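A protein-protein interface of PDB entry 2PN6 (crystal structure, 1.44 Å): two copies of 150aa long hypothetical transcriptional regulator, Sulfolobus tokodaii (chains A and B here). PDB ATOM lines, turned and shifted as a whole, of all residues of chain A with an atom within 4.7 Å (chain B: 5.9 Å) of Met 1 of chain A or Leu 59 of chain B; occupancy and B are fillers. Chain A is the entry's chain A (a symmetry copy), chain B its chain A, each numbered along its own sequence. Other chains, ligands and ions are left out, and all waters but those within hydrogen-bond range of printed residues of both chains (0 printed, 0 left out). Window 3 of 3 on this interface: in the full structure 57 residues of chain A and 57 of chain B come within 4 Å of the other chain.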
ATOM      1  N   MET A   1      34.447  21.446 -27.356  1.00  0.00           N
ATOM      2  CA  MET A   1      34.225  20.295 -28.276  1.00  0.00           C
ATOM      3  C   MET A   1      34.504  20.696 -29.716  1.00  0.00           C
ATOM      4  O   MET A   1      34.556  21.881 -30.041  1.00  0.00           O
ATOM      5  CB  MET A   1      32.777  19.808 -28.194  1.00  0.00           C
ATOM      6  CG  MET A   1      32.255  19.541 -26.799  1.00  0.00           C
ATOM      7  SD  MET A   1      30.614  18.786 -26.871  1.00  0.00           S
ATOM      8  CE  MET A   1      29.876  19.675 -28.244  1.00  0.00           C
ATOM      9  N   ASP A   2      34.678  19.697 -30.576  1.00  0.00           N
ATOM     10  CA  ASP A   2      34.920  19.940 -31.991  1.00  0.00           C
ATOM     11  C   ASP A   2      33.972  19.108 -32.848  1.00  0.00           C
ATOM     12  O   ASP A   2      33.046  18.477 -32.337  1.00  0.00           O
ATOM     13  CB  ASP A   2      36.375  19.629 -32.363  1.00  0.00           C
ATOM     14  CG  ASP A   2      36.818  18.256 -31.906  1.00  0.00           C
ATOM     15  OD1 ASP A   2      35.998  17.317 -31.948  1.00  0.00           O
ATOM     16  OD2 ASP A   2      37.997  18.113 -31.516  1.00  0.00           O
ATOM     17  N   ASP A   5      33.757  15.436 -31.835  1.00  0.00           N
ATOM     18  CA  ASP A   5      32.991  15.184 -30.620  1.00  0.00           C
ATOM     19  C   ASP A   5      31.506  15.110 -30.946  1.00  0.00           C
ATOM     20  O   ASP A   5      30.784  14.274 -30.401  1.00  0.00           O
ATOM     21  CB  ASP A   5      33.230  16.283 -29.579  1.00  0.00           C
ATOM     22  CG  ASP A   5      34.612  16.210 -28.959  1.00  0.00           C
ATOM     23  OD1 ASP A   5      35.034  15.100 -28.578  1.00  0.00           O
ATOM     24  OD2 ASP A   5      35.272  17.265 -28.842  1.00  0.00           O
ATOM     25  N   LEU A   6      31.051  15.983 -31.838  1.00  0.00           N
ATOM     26  CA  LEU A   6      29.646  15.999 -32.225  1.00  0.00           C
ATOM     27  C   LEU A   6      29.241  14.710 -32.929  1.00  0.00           C
ATOM     28  O   LEU A   6      28.148  14.191 -32.705  1.00  0.00           O
ATOM     29  CB  LEU A   6      29.353  17.200 -33.128  1.00  0.00           C
ATOM     30  CG  LEU A   6      29.424  18.569 -32.450  1.00  0.00           C
ATOM     31  CD1 LEU A   6      29.034  19.648 -33.448  1.00  0.00           C
ATOM     32  CD2 LEU A   6      28.488  18.598 -31.249  1.00  0.00           C
ATOM     33  N   LEU A   9      28.915  12.064 -30.286  1.00  0.00           N
ATOM     34  CA  LEU A   9      27.681  12.287 -29.547  1.00  0.00           C
ATOM     35  C   LEU A   9      26.451  11.907 -30.367  1.00  0.00           C
ATOM     36  O   LEU A   9      25.473  11.393 -29.825  1.00  0.00           O
ATOM     37  CB  LEU A   9      27.573  13.756 -29.126  1.00  0.00           C
ATOM     38  CG  LEU A   9      28.584  14.251 -28.088  1.00  0.00           C
ATOM     39  CD1 LEU A   9      28.399  15.745 -27.875  1.00  0.00           C
ATOM     40  CD2 LEU A   9      28.394  13.493 -26.778  1.00  0.00           C
ATOM     41  N   LEU A  41      34.371  14.073 -22.411  1.00  0.00           N
ATOM     42  CA  LEU A  41      33.006  14.574 -22.529  1.00  0.00           C
ATOM     43  C   LEU A  41      32.223  14.285 -21.254  1.00  0.00           C
ATOM     44  O   LEU A  41      31.361  15.070 -20.853  1.00  0.00           O
ATOM     45  CB  LEU A  41      32.308  13.933 -23.731  1.00  0.00           C
ATOM     46  CG  LEU A  41      32.833  14.382 -25.098  1.00  0.00           C
ATOM     47  CD1 LEU A  41      32.314  13.456 -26.179  1.00  0.00           C
ATOM     48  CD2 LEU A  41      32.408  15.816 -25.367  1.00  0.00           C
ATOM     49  N   VAL A  46      29.338  17.031 -20.461  1.00  0.00           N
ATOM     50  CA  VAL A  46      28.560  17.011 -21.696  1.00  0.00           C
ATOM     51  C   VAL A  46      27.705  15.748 -21.688  1.00  0.00           C
ATOM     52  O   VAL A  46      26.516  15.782 -22.002  1.00  0.00           O
ATOM     53  CB  VAL A  46      29.472  17.017 -22.935  1.00  0.00           C
ATOM     54  CG1 VAL A  46      28.637  16.878 -24.197  1.00  0.00           C
ATOM     55  CG2 VAL A  46      30.274  18.313 -22.975  1.00  0.00           C
ATOM     56  N   VAL A 148      19.469  15.019 -29.331  1.00  0.00           N
ATOM     57  CA  VAL A 148      19.806  16.427 -29.145  1.00  0.00           C
ATOM     58  C   VAL A 148      20.501  17.028 -30.363  1.00  0.00           C
ATOM     59  O   VAL A 148      20.536  18.242 -30.526  1.00  0.00           O
ATOM     60  CB  VAL A 148      20.700  16.624 -27.907  1.00  0.00           C
ATOM     61  CG1 VAL A 148      19.893  16.385 -26.635  1.00  0.00           C
ATOM     62  CG2 VAL A 148      21.876  15.670 -27.969  1.00  0.00           C
ATOM     63  N   ILE A 149      21.049  16.164 -31.211  1.00  0.00           N
ATOM     64  CA  ILE A 149      21.737  16.563 -32.435  1.00  0.00           C
ATOM     65  C   ILE A 149      20.968  15.991 -33.622  1.00  0.00           C
ATOM     66  O   ILE A 149      20.961  14.779 -33.832  1.00  0.00           O
ATOM     67  CB  ILE A 149      23.175  15.993 -32.469  1.00  0.00           C
ATOM     68  CG1 ILE A 149      23.951  16.479 -31.245  1.00  0.00           C
ATOM     69  CG2 ILE A 149      23.872  16.403 -33.753  1.00  0.00           C
ATOM     70  CD1 ILE A 149      25.283  15.783 -31.069  1.00  0.00           C
ATOM     71  N   ILE B  54      22.780  13.498 -22.962  1.00  0.00           N
ATOM     72  CA  ILE B  54      23.609  14.652 -23.275  1.00  0.00           C
ATOM     73  C   ILE B  54      22.955  15.928 -22.777  1.00  0.00           C
ATOM     74  O   ILE B  54      21.765  16.154 -23.003  1.00  0.00           O
ATOM     75  CB  ILE B  54      23.837  14.767 -24.793  1.00  0.00           C
ATOM     76  CG1 ILE B  54      24.543  13.507 -25.300  1.00  0.00           C
ATOM     77  CG2 ILE B  54      24.656  16.015 -25.109  1.00  0.00           C
ATOM     78  CD1 ILE B  54      24.564  13.379 -26.799  1.00  0.00           C
ATOM     79  N   ASN B  55      23.739  16.750 -22.092  1.00  0.00           N
ATOM     80  CA  ASN B  55      23.240  18.011 -21.561  1.00  0.00           C
ATOM     81  C   ASN B  55      22.989  18.974 -22.717  1.00  0.00           C
ATOM     82  O   ASN B  55      23.929  19.454 -23.353  1.00  0.00           O
ATOM     83  CB  ASN B  55      24.259  18.609 -20.591  1.00  0.00           C
ATOM     84  CG  ASN B  55      23.790  19.916 -19.990  1.00  0.00           C
ATOM     85  OD1 ASN B  55      22.703  19.994 -19.422  1.00  0.00           O
ATOM     86  ND2 ASN B  55      24.611  20.951 -20.110  1.00  0.00           N
ATOM     87  N   PRO B  56      21.711  19.267 -23.008  1.00  0.00           N
ATOM     88  CA  PRO B  56      21.364  20.179 -24.101  1.00  0.00           C
ATOM     89  C   PRO B  56      22.053  21.535 -23.990  1.00  0.00           C
ATOM     90  O   PRO B  56      22.369  22.160 -24.997  1.00  0.00           O
ATOM     91  CB  PRO B  56      19.847  20.285 -23.989  1.00  0.00           C
ATOM     92  CG  PRO B  56      19.467  18.929 -23.485  1.00  0.00           C
ATOM     93  CD  PRO B  56      20.492  18.711 -22.395  1.00  0.00           C
ATOM     94  N   ALA B  57      22.285  21.983 -22.762  1.00  0.00           N
ATOM     95  CA  ALA B  57      22.942  23.264 -22.545  1.00  0.00           C
ATOM     96  C   ALA B  57      24.352  23.252 -23.129  1.00  0.00           C
ATOM     97  O   ALA B  57      24.846  24.276 -23.605  1.00  0.00           O
ATOM     98  CB  ALA B  57      22.990  23.581 -21.054  1.00  0.00           C
ATOM     99  N   SER B  58      24.995  22.086 -23.101  1.00  0.00           N
ATOM    100  CA  SER B  58      26.348  21.944 -23.630  1.00  0.00           C
ATOM    101  C   SER B  58      26.369  22.147 -25.140  1.00  0.00           C
ATOM    102  O   SER B  58      27.415  22.434 -25.723  1.00  0.00           O
ATOM    103  CB  SER B  58      26.908  20.559 -23.291  1.00  0.00           C
ATOM    104  OG  SER B  58      26.933  20.351 -21.891  1.00  0.00           O
ATOM    105  N   LEU B  59      25.208  21.989 -25.768  1.00  0.00           N
ATOM    106  CA  LEU B  59      25.077  22.164 -27.209  1.00  0.00           C
ATOM    107  C   LEU B  59      24.423  23.510 -27.512  1.00  0.00           C
ATOM    108  O   LEU B  59      23.970  23.759 -28.629  1.00  0.00           O
ATOM    109  CB  LEU B  59      24.237  21.032 -27.804  1.00  0.00           C
ATOM    110  CG  LEU B  59      24.840  19.630 -27.706  1.00  0.00           C
ATOM    111  CD1 LEU B  59      23.815  18.599 -28.148  1.00  0.00           C
ATOM    112  CD2 LEU B  59      26.092  19.550 -28.563  1.00  0.00           C
ATOM    113  N   ASN B  60      24.370  24.370 -26.499  1.00  0.00           N
ATOM    114  CA  ASN B  60      23.786  25.702 -26.641  1.00  0.00           C
ATOM    115  C   ASN B  60      22.300  25.691 -26.997  1.00  0.00           C
ATOM    116  O   ASN B  60      21.796  26.653 -27.574  1.00  0.00           O
ATOM    117  CB  ASN B  60      24.556  26.496 -27.699  1.00  0.00           C
ATOM    118  CG  ASN B  60      26.002  26.742 -27.305  1.00  0.00           C
ATOM    119  OD1 ASN B  60      26.898  26.721 -28.150  1.00  0.00           O
ATOM    120  ND2 ASN B  60      26.232  26.992 -26.022  1.00  0.00           N
ATOM    121  N   LEU B  61      21.605  24.605 -26.668  1.00  0.00           N
ATOM    122  CA  LEU B  61      20.172  24.503 -26.948  1.00  0.00           C
ATOM    123  C   LEU B  61      19.447  25.268 -25.848  1.00  0.00           C
ATOM    124  O   LEU B  61      18.945  24.684 -24.884  1.00  0.00           O
ATOM    125  CB  LEU B  61      19.746  23.035 -26.968  1.00  0.00           C
ATOM    126  CG  LEU B  61      20.330  22.242 -28.141  1.00  0.00           C
ATOM    127  CD1 LEU B  61      20.141  20.749 -27.913  1.00  0.00           C
ATOM    128  CD2 LEU B  61      19.667  22.687 -29.435  1.00  0.00           C
ATOM    129  N   LYS B 110      19.007  26.421 -30.827  1.00  0.00           N
ATOM    130  CA  LYS B 110      20.059  27.211 -30.206  1.00  0.00           C
ATOM    131  C   LYS B 110      19.668  28.669 -30.047  1.00  0.00           C
ATOM    132  O   LYS B 110      20.006  29.302 -29.047  1.00  0.00           O
ATOM    133  CB  LYS B 110      21.352  27.109 -31.020  1.00  0.00           C
ATOM    134  CG  LYS B 110      22.002  25.739 -30.956  1.00  0.00           C
ATOM    135  CD  LYS B 110      23.215  25.646 -31.868  1.00  0.00           C
ATOM    136  CE  LYS B 110      23.927  24.315 -31.697  1.00  0.00           C
ATOM    137  NZ  LYS B 110      24.989  24.099 -32.720  1.00  0.00           N
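N of Asn 55 of chain B is in hydrogen-bond range of O of Val 46 of chain A (2.9 Å).
Met 1 of chain A touches Leu 59 of chain B.
Leu 59 of chain B touches Leu 6 of chain A.
Leu 9 of chain A touches Ile 54 of chain B.
Val 46 of chain A touches Ile 54 of chain B.
Val 46 of chain A touches Ser 58 of chain B.
CG2 of Val 148 of chain A touches CD1 of Ile 54 of chain B, at 3.7 Å.
CD1 of Leu 59 of chain B touches CG2 of Val 148 of chain A (3.5 Å).
Val 148 of chain A touches Leu 61 of chain B.
Ile 149 of chain A touches Leu 59 of chain B (CG1 to CD1, 3.8 Å).
No position is printed for both chains.
Hydrophobic or aromatic side chains of chain A that line the printed part of chain B: Met 1, Leu 6, Leu 9, Val 148 and Ile 149.
Printed residues of chain B that touch a printed residue of chain A: Ile 54, Asn 55, Ser 58, Leu 59 and Leu 61.
Among the printed residues, no Asp or Glu carboxylate lies within 4 Å of a Lys or Arg side-chain nitrogen of the other chain.
Met 1 of chain A touches just one residue of chain B: Leu 59.
Of the printed residues of chain B, Leu 9 of chain A touches Ile 54 (3.7 Å).
Of the printed residues of chain A, Ile 54 of chain B touches Leu 9, Val 46 and Val 148.
Of the printed residues of chain A, Asn 55 of chain B touches Val 46.
Printed residues of chain A within 4 Å of Ser 58 of chain B: Val 46.
Of chain A, only Met 1, Leu 6, Val 148 and Ile 149 come within 4 Å of Leu 59 of chain B.
Of the printed residues of chain A, Leu 61 of chain B touches Val 148.
ND2 of Asn 55 of chain B lies within hydrogen-bond range of OG of Ser 58 of chain B, at 3.0 Å.
The backbone carbonyl oxygen (O) of Leu 41 of chain A sits at hydrogen-bond distance from the backbone NH (N) of Val 46 of chain A (2.8 Å).
O of Pro 56 of chain B is in hydrogen-bond range of N of Leu 61 of chain B (3.1 Å).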
